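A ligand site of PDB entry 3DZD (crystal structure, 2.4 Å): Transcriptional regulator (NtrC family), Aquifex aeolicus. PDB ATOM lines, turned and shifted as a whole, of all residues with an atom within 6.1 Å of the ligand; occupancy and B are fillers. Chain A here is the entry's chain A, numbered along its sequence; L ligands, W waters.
N of Val 347 is in hydrogen-bond range of O of Gly 162, 2.9 Å away. The backbone carbonyl oxygen of Thr 163 lies within hydrogen-bond range of the guanidinium group of Arg 304, at 3.1 Å. The backbone NH (N) of Arg 348 sits at hydrogen-bond distance from the backbone carbonyl oxygen (O) of Gly 162 (3.5 Å). The side-chain hydroxyl (OG1) of Thr 163 is in hydrogen-bond range of the backbone carbonyl oxygen (O) of Glu 160 (2.8 Å).
Water W3 lies within hydrogen-bond range of O9 of the ligand and NZ of Lys 351. Water W4 lies within hydrogen-bond range of O of Thr 163, NH1 of Arg 304 and N2 of the ligand. Water W5 bridges an oxygen (O10) of the ligand and the side-chain hydroxyl (OH) of Tyr 314.
Glu 130 touches the ligand. Phe 131 touches the ligand. Ile 167 touches the ligand. Leu 311 touches the ligand. Tyr 314 touches the ligand. CZ of Phe 315 touches N5 of the ligand, at 3.9 Å. CG1 of Val 347 touches C6 of the ligand, at 3.3 Å. Hydrophobic or aromatic side chains that line the ligand: Phe 131, Val 132, Ile 167, Leu 311, Tyr 314, Phe 315 and Val 347.
The backbone NH (N) of Gly 162 is in hydrogen-bond range of an oxygen (O2) of the ligand, at 3.2 Å. The side-chain amino group of Lys 351 lies within hydrogen-bond range of an oxygen (O9) of the ligand (3.2 Å). N of Gly 164 lies within hydrogen-bond range of O3 of the ligand. The guanidinium group of Arg 348 is in salt-bridge range of an oxygen (O2) of the ligand (3.8 Å). The backbone NH of Thr 163 sits at hydrogen-bond distance from an oxygen (O3) of the ligand (2.9 Å). N of Lys 165 lies within hydrogen-bond range of O3 of the ligand, 3.0 Å away. The backbone NH of Glu 166 lies within hydrogen-bond range of an oxygen (O1) of the ligand, at 3.3 Å. A nitrogen (N3) of the ligand sits at hydrogen-bond distance from the backbone carbonyl oxygen of Val 132 (3.2 Å). The backbone NH (N) of Val 132 is in hydrogen-bond range of a nitrogen (N4) of the ligand (2.9 Å).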
ATOM      1  N   GLU A 130     -14.198  -2.969  31.810  1.00  0.00           N
ATOM      2  CA  GLU A 130     -13.571  -4.028  32.592  1.00  0.00           C
ATOM      3  C   GLU A 130     -12.549  -4.764  31.743  1.00  0.00           C
ATOM      4  O   GLU A 130     -12.868  -5.306  30.676  1.00  0.00           O
ATOM      5  CB  GLU A 130     -14.635  -5.009  33.085  1.00  0.00           C
ATOM      6  CG  GLU A 130     -15.796  -4.356  33.817  1.00  0.00           C
ATOM      7  CD  GLU A 130     -15.505  -4.066  35.278  1.00  0.00           C
ATOM      8  OE1 GLU A 130     -14.451  -4.526  35.772  1.00  0.00           O
ATOM      9  OE2 GLU A 130     -16.327  -3.387  35.924  1.00  0.00           O
ATOM     10  N   PHE A 131     -11.308  -4.790  32.215  1.00  0.00           N
ATOM     11  CA  PHE A 131     -10.255  -5.496  31.524  1.00  0.00           C
ATOM     12  C   PHE A 131      -9.549  -6.369  32.535  1.00  0.00           C
ATOM     13  O   PHE A 131      -8.560  -5.965  33.128  1.00  0.00           O
ATOM     14  CB  PHE A 131      -9.282  -4.511  30.897  1.00  0.00           C
ATOM     15  CG  PHE A 131      -8.250  -5.157  30.042  1.00  0.00           C
ATOM     16  CD1 PHE A 131      -7.024  -4.541  29.822  1.00  0.00           C
ATOM     17  CD2 PHE A 131      -8.495  -6.399  29.465  1.00  0.00           C
ATOM     18  CE1 PHE A 131      -6.072  -5.137  29.018  1.00  0.00           C
ATOM     19  CE2 PHE A 131      -7.544  -7.012  28.675  1.00  0.00           C
ATOM     20  CZ  PHE A 131      -6.327  -6.377  28.450  1.00  0.00           C
ATOM     21  N   VAL A 132     -10.072  -7.575  32.735  1.00  0.00           N
ATOM     22  CA  VAL A 132      -9.646  -8.397  33.858  1.00  0.00           C
ATOM     23  C   VAL A 132      -8.442  -9.269  33.524  1.00  0.00           C
ATOM     24  O   VAL A 132      -8.401  -9.899  32.463  1.00  0.00           O
ATOM     25  CB  VAL A 132     -10.801  -9.261  34.380  1.00  0.00           C
ATOM     26  CG1 VAL A 132     -10.314 -10.202  35.465  1.00  0.00           C
ATOM     27  CG2 VAL A 132     -11.914  -8.355  34.891  1.00  0.00           C
ATOM     28  N   GLY A 133      -7.470  -9.304  34.436  1.00  0.00           N
ATOM     29  CA  GLY A 133      -6.287 -10.104  34.261  1.00  0.00           C
ATOM     30  C   GLY A 133      -5.097  -9.601  35.050  1.00  0.00           C
ATOM     31  O   GLY A 133      -4.813  -8.398  35.054  1.00  0.00           O
ATOM     32  N   GLU A 160      -5.827 -14.370  19.030  1.00  0.00           N
ATOM     33  CA  GLU A 160      -6.833 -15.328  18.623  1.00  0.00           C
ATOM     34  C   GLU A 160      -8.235 -14.772  18.855  1.00  0.00           C
ATOM     35  O   GLU A 160      -8.399 -13.724  19.500  1.00  0.00           O
ATOM     36  CB  GLU A 160      -6.665 -16.627  19.390  1.00  0.00           C
ATOM     37  CG  GLU A 160      -5.422 -17.400  19.037  1.00  0.00           C
ATOM     38  CD  GLU A 160      -5.373 -18.782  19.687  1.00  0.00           C
ATOM     39  OE1 GLU A 160      -6.240 -19.049  20.554  1.00  0.00           O
ATOM     40  OE2 GLU A 160      -4.470 -19.577  19.339  1.00  0.00           O
ATOM     41  N   SER A 161      -9.233 -15.467  18.337  1.00  0.00           N
ATOM     42  CA  SER A 161     -10.615 -15.022  18.467  1.00  0.00           C
ATOM     43  C   SER A 161     -11.022 -15.031  19.925  1.00  0.00           C
ATOM     44  O   SER A 161     -10.646 -15.934  20.677  1.00  0.00           O
ATOM     45  CB  SER A 161     -11.542 -15.914  17.661  1.00  0.00           C
ATOM     46  OG  SER A 161     -11.175 -15.886  16.301  1.00  0.00           O
ATOM     47  N   GLY A 162     -11.786 -14.015  20.313  1.00  0.00           N
ATOM     48  CA  GLY A 162     -12.284 -13.902  21.666  1.00  0.00           C
ATOM     49  C   GLY A 162     -11.243 -13.634  22.723  1.00  0.00           C
ATOM     50  O   GLY A 162     -11.439 -14.016  23.876  1.00  0.00           O
ATOM     51  N   THR A 163     -10.147 -12.970  22.382  1.00  0.00           N
ATOM     52  CA  THR A 163      -9.126 -12.641  23.387  1.00  0.00           C
ATOM     53  C   THR A 163      -9.222 -11.210  23.949  1.00  0.00           C
ATOM     54  O   THR A 163      -8.373 -10.786  24.712  1.00  0.00           O
ATOM     55  CB  THR A 163      -7.696 -12.864  22.868  1.00  0.00           C
ATOM     56  OG1 THR A 163      -7.552 -12.182  21.638  1.00  0.00           O
ATOM     57  CG2 THR A 163      -7.430 -14.330  22.648  1.00  0.00           C
ATOM     58  N   GLY A 164     -10.267 -10.473  23.575  1.00  0.00           N
ATOM     59  CA  GLY A 164     -10.472  -9.151  24.159  1.00  0.00           C
ATOM     60  C   GLY A 164      -9.900  -8.012  23.340  1.00  0.00           C
ATOM     61  O   GLY A 164      -9.654  -6.932  23.867  1.00  0.00           O
ATOM     62  N   LYS A 165      -9.701  -8.246  22.051  1.00  0.00           N
ATOM     63  CA  LYS A 165      -9.118  -7.239  21.176  1.00  0.00           C
ATOM     64  C   LYS A 165      -9.935  -5.938  21.133  1.00  0.00           C
ATOM     65  O   LYS A 165      -9.360  -4.858  21.069  1.00  0.00           O
ATOM     66  CB  LYS A 165      -8.908  -7.810  19.778  1.00  0.00           C
ATOM     67  CG  LYS A 165      -7.793  -8.863  19.723  1.00  0.00           C
ATOM     68  CD  LYS A 165      -7.713  -9.530  18.354  1.00  0.00           C
ATOM     69  CE  LYS A 165      -8.919 -10.415  18.127  1.00  0.00           C
ATOM     70  NZ  LYS A 165      -8.959 -10.897  16.722  1.00  0.00           N
ATOM     71  N   GLU A 166     -11.254  -6.039  21.174  1.00  0.00           N
ATOM     72  CA  GLU A 166     -12.090  -4.851  21.182  1.00  0.00           C
ATOM     73  C   GLU A 166     -11.991  -4.072  22.489  1.00  0.00           C
ATOM     74  O   GLU A 166     -11.988  -2.829  22.497  1.00  0.00           O
ATOM     75  CB  GLU A 166     -13.559  -5.175  20.859  1.00  0.00           C
ATOM     76  CG  GLU A 166     -14.495  -4.008  21.136  1.00  0.00           C
ATOM     77  CD  GLU A 166     -15.915  -4.198  20.604  1.00  0.00           C
ATOM     78  OE1 GLU A 166     -16.094  -4.803  19.518  1.00  0.00           O
ATOM     79  OE2 GLU A 166     -16.846  -3.709  21.275  1.00  0.00           O
ATOM     80  N   ILE A 167     -11.916  -4.776  23.601  1.00  0.00           N
ATOM     81  CA  ILE A 167     -11.736  -4.112  24.889  1.00  0.00           C
ATOM     82  C   ILE A 167     -10.490  -3.253  24.877  1.00  0.00           C
ATOM     83  O   ILE A 167     -10.505  -2.115  25.342  1.00  0.00           O
ATOM     84  CB  ILE A 167     -11.609  -5.091  26.053  1.00  0.00           C
ATOM     85  CG1 ILE A 167     -12.935  -5.829  26.277  1.00  0.00           C
ATOM     86  CG2 ILE A 167     -11.190  -4.353  27.296  1.00  0.00           C
ATOM     87  CD1 ILE A 167     -12.948  -6.666  27.546  1.00  0.00           C
ATOM     88  N   PHE A 227     -12.315   1.386  14.710  1.00  0.00           N
ATOM     89  CA  PHE A 227     -11.818   0.040  15.007  1.00  0.00           C
ATOM     90  C   PHE A 227     -12.225  -0.926  13.899  1.00  0.00           C
ATOM     91  O   PHE A 227     -13.404  -1.213  13.710  1.00  0.00           O
ATOM     92  CB  PHE A 227     -12.332  -0.457  16.364  1.00  0.00           C
ATOM     93  CG  PHE A 227     -11.944  -1.888  16.698  1.00  0.00           C
ATOM     94  CD1 PHE A 227     -10.622  -2.283  16.721  1.00  0.00           C
ATOM     95  CD2 PHE A 227     -12.919  -2.831  17.011  1.00  0.00           C
ATOM     96  CE1 PHE A 227     -10.275  -3.585  17.040  1.00  0.00           C
ATOM     97  CE2 PHE A 227     -12.572  -4.132  17.330  1.00  0.00           C
ATOM     98  CZ  PHE A 227     -11.250  -4.510  17.340  1.00  0.00           C
ATOM     99  N   ASP A 229     -12.299  -4.494  12.970  1.00  0.00           N
ATOM    100  CA  ASP A 229     -12.181  -5.870  13.436  1.00  0.00           C
ATOM    101  C   ASP A 229     -11.919  -6.825  12.264  1.00  0.00           C
ATOM    102  O   ASP A 229     -12.571  -6.741  11.231  1.00  0.00           O
ATOM    103  CB  ASP A 229     -13.427  -6.299  14.212  1.00  0.00           C
ATOM    104  CG  ASP A 229     -13.120  -7.368  15.270  1.00  0.00           C
ATOM    105  OD1 ASP A 229     -12.057  -8.019  15.190  1.00  0.00           O
ATOM    106  OD2 ASP A 229     -13.957  -7.553  16.192  1.00  0.00           O
ATOM    107  N   LEU A 298      -2.183  -9.917  22.096  1.00  0.00           N
ATOM    108  CA  LEU A 298      -2.937 -10.513  23.208  1.00  0.00           C
ATOM    109  C   LEU A 298      -2.780 -12.023  23.191  1.00  0.00           C
ATOM    110  O   LEU A 298      -3.169 -12.665  22.234  1.00  0.00           O
ATOM    111  CB  LEU A 298      -4.429 -10.186  23.097  1.00  0.00           C
ATOM    112  CG  LEU A 298      -4.827  -8.721  23.001  1.00  0.00           C
ATOM    113  CD1 LEU A 298      -6.347  -8.555  23.114  1.00  0.00           C
ATOM    114  CD2 LEU A 298      -4.099  -7.913  24.068  1.00  0.00           C
ATOM    115  N   ARG A 304      -2.558 -17.589  30.085  1.00  0.00           N
ATOM    116  CA  ARG A 304      -2.721 -16.500  31.048  1.00  0.00           C
ATOM    117  C   ARG A 304      -2.806 -16.957  32.499  1.00  0.00           C
ATOM    118  O   ARG A 304      -3.268 -16.222  33.378  1.00  0.00           O
ATOM    119  CB  ARG A 304      -3.946 -15.666  30.707  1.00  0.00           C
ATOM    120  CG  ARG A 304      -3.882 -15.063  29.330  1.00  0.00           C
ATOM    121  CD  ARG A 304      -4.868 -13.949  29.220  1.00  0.00           C
ATOM    122  NE  ARG A 304      -5.132 -13.604  27.831  1.00  0.00           N
ATOM    123  CZ  ARG A 304      -6.157 -12.860  27.436  1.00  0.00           C
ATOM    124  NH1 ARG A 304      -7.017 -12.406  28.348  1.00  0.00           N
ATOM    125  NH2 ARG A 304      -6.331 -12.579  26.141  1.00  0.00           N
ATOM    126  N   LEU A 311     -11.452 -14.367  35.599  1.00  0.00           N
ATOM    127  CA  LEU A 311     -12.476 -14.079  34.629  1.00  0.00           C
ATOM    128  C   LEU A 311     -13.772 -14.816  34.964  1.00  0.00           C
ATOM    129  O   LEU A 311     -14.875 -14.252  34.858  1.00  0.00           O
ATOM    130  CB  LEU A 311     -11.977 -14.444  33.232  1.00  0.00           C
ATOM    131  CG  LEU A 311     -10.963 -13.446  32.674  1.00  0.00           C
ATOM    132  CD1 LEU A 311     -10.133 -14.015  31.529  1.00  0.00           C
ATOM    133  CD2 LEU A 311     -11.681 -12.159  32.236  1.00  0.00           C
ATOM    134  N   TYR A 314     -15.484 -13.159  37.725  1.00  0.00           N
ATOM    135  CA  TYR A 314     -16.011 -11.886  37.259  1.00  0.00           C
ATOM    136  C   TYR A 314     -17.322 -12.100  36.496  1.00  0.00           C
ATOM    137  O   TYR A 314     -18.276 -11.323  36.645  1.00  0.00           O
ATOM    138  CB  TYR A 314     -14.967 -11.181  36.390  1.00  0.00           C
ATOM    139  CG  TYR A 314     -15.484 -10.059  35.505  1.00  0.00           C
ATOM    140  CD1 TYR A 314     -15.600  -8.758  35.980  1.00  0.00           C
ATOM    141  CD2 TYR A 314     -15.836 -10.302  34.187  1.00  0.00           C
ATOM    142  CE1 TYR A 314     -16.057  -7.735  35.164  1.00  0.00           C
ATOM    143  CE2 TYR A 314     -16.293  -9.301  33.366  1.00  0.00           C
ATOM    144  CZ  TYR A 314     -16.408  -8.015  33.864  1.00  0.00           C
ATOM    145  OH  TYR A 314     -16.865  -7.028  33.025  1.00  0.00           O
ATOM    146  N   PHE A 315     -17.368 -13.152  35.679  1.00  0.00           N
ATOM    147  CA  PHE A 315     -18.569 -13.429  34.899  1.00  0.00           C
ATOM    148  C   PHE A 315     -19.674 -14.021  35.776  1.00  0.00           C
ATOM    149  O   PHE A 315     -20.836 -13.673  35.660  1.00  0.00           O
ATOM    150  CB  PHE A 315     -18.267 -14.339  33.697  1.00  0.00           C
ATOM    151  CG  PHE A 315     -17.452 -13.666  32.611  1.00  0.00           C
ATOM    152  CD1 PHE A 315     -17.889 -12.462  32.046  1.00  0.00           C
ATOM    153  CD2 PHE A 315     -16.260 -14.224  32.156  1.00  0.00           C
ATOM    154  CE1 PHE A 315     -17.145 -11.832  31.060  1.00  0.00           C
ATOM    155  CE2 PHE A 315     -15.526 -13.606  31.162  1.00  0.00           C
ATOM    156  CZ  PHE A 315     -15.953 -12.410  30.609  1.00  0.00           C
ATOM    157  N   VAL A 347     -11.834 -16.217  25.690  1.00  0.00           N
ATOM    158  CA  VAL A 347     -12.655 -15.567  26.718  1.00  0.00           C
ATOM    159  C   VAL A 347     -14.116 -15.624  26.303  1.00  0.00           C
ATOM    160  O   VAL A 347     -15.023 -15.716  27.125  1.00  0.00           O
ATOM    161  CB  VAL A 347     -12.242 -14.104  26.958  1.00  0.00           C
ATOM    162  CG1 VAL A 347     -13.153 -13.445  27.983  1.00  0.00           C
ATOM    163  CG2 VAL A 347     -10.801 -14.021  27.408  1.00  0.00           C
ATOM    164  N   ARG A 348     -14.328 -15.590  24.993  1.00  0.00           N
ATOM    165  CA  ARG A 348     -15.659 -15.662  24.438  1.00  0.00           C
ATOM    166  C   ARG A 348     -16.292 -17.008  24.818  1.00  0.00           C
ATOM    167  O   ARG A 348     -17.451 -17.068  25.228  1.00  0.00           O
ATOM    168  CB  ARG A 348     -15.573 -15.493  22.920  1.00  0.00           C
ATOM    169  CG  ARG A 348     -16.875 -15.371  22.206  1.00  0.00           C
ATOM    170  CD  ARG A 348     -16.601 -14.763  20.848  1.00  0.00           C
ATOM    171  NE  ARG A 348     -15.958 -15.731  19.973  1.00  0.00           N
ATOM    172  CZ  ARG A 348     -15.272 -15.396  18.880  1.00  0.00           C
ATOM    173  NH1 ARG A 348     -15.139 -14.114  18.554  1.00  0.00           N
ATOM    174  NH2 ARG A 348     -14.719 -16.340  18.133  1.00  0.00           N
ATOM    175  N   LYS A 351     -16.884 -17.001  28.767  1.00  0.00           N
ATOM    176  CA  LYS A 351     -17.997 -16.164  29.189  1.00  0.00           C
ATOM    177  C   LYS A 351     -19.304 -16.898  28.954  1.00  0.00           C
ATOM    178  O   LYS A 351     -20.131 -17.035  29.856  1.00  0.00           O
ATOM    179  CB  LYS A 351     -18.015 -14.833  28.426  1.00  0.00           C
ATOM    180  CG  LYS A 351     -18.999 -13.841  29.012  1.00  0.00           C
ATOM    181  CD  LYS A 351     -19.167 -12.577  28.171  1.00  0.00           C
ATOM    182  CE  LYS A 351     -19.978 -12.862  26.913  1.00  0.00           C
ATOM    183  NZ  LYS A 351     -20.606 -11.609  26.400  1.00  0.00           N
HETATM  184  P1  LIG L   1     -12.294 -10.383  20.313  1.00  0.00           P
HETATM  185  O1  LIG L   1     -12.592  -8.899  20.204  1.00  0.00           O
HETATM  186  O2  LIG L   1     -12.773 -11.208  19.148  1.00  0.00           O
HETATM  187  O3  LIG L   1     -10.872 -10.695  20.666  1.00  0.00           O
HETATM  188  P2  LIG L   1     -14.231 -10.167  22.463  1.00  0.00           P
HETATM  189  O4  LIG L   1     -13.573  -9.277  23.483  1.00  0.00           O
HETATM  190  O5  LIG L   1     -15.236  -9.526  21.527  1.00  0.00           O
HETATM  191  O6  LIG L   1     -13.079 -10.942  21.622  1.00  0.00           O
HETATM  192  O7  LIG L   1     -14.973 -11.356  23.240  1.00  0.00           O
HETATM  193  C1  LIG L   1     -14.789 -11.548  24.631  1.00  0.00           C
HETATM  194  C2  LIG L   1     -16.079 -11.356  25.410  1.00  0.00           C
HETATM  195  O8  LIG L   1     -15.716 -11.408  26.783  1.00  0.00           O
HETATM  196  C3  LIG L   1     -16.616  -9.959  25.225  1.00  0.00           C
HETATM  197  O9  LIG L   1     -17.985  -9.940  25.630  1.00  0.00           O
HETATM  198  C4  LIG L   1     -15.868  -9.105  26.212  1.00  0.00           C
HETATM  199  O10 LIG L   1     -16.822  -8.191  26.762  1.00  0.00           O
HETATM  200  C5  LIG L   1     -15.471 -10.089  27.285  1.00  0.00           C
HETATM  201  N1  LIG L   1     -14.031  -9.987  27.620  1.00  0.00           N
HETATM  202  C6  LIG L   1     -13.011 -10.328  26.819  1.00  0.00           C
HETATM  203  N2  LIG L   1     -11.821 -10.147  27.414  1.00  0.00           N
HETATM  204  C7  LIG L   1     -12.070  -9.669  28.647  1.00  0.00           C
HETATM  205  C8  LIG L   1     -11.250  -9.249  29.808  1.00  0.00           C
HETATM  206  N3  LIG L   1      -9.890  -9.315  29.747  1.00  0.00           N
HETATM  207  N4  LIG L   1     -11.890  -8.811  30.896  1.00  0.00           N
HETATM  208  C9  LIG L   1     -13.240  -8.748  30.946  1.00  0.00           C
HETATM  209  N5  LIG L   1     -14.051  -9.108  29.937  1.00  0.00           N
HETATM  210  C10 LIG L   1     -13.531  -9.569  28.782  1.00  0.00           C
HETATM  211  O   HOH W   1     -12.937 -11.385  16.412  1.00  0.00           O
HETATM  212  O   HOH W   2     -18.407 -12.528  23.335  1.00  0.00           O
HETATM  213  O   HOH W   3     -20.039 -10.184  23.501  1.00  0.00           O
HETATM  214  O   HOH W   4      -8.879 -10.473  27.167  1.00  0.00           O
HETATM  215  O   HOH W   5     -16.838  -7.793  29.811  1.00  0.00           O
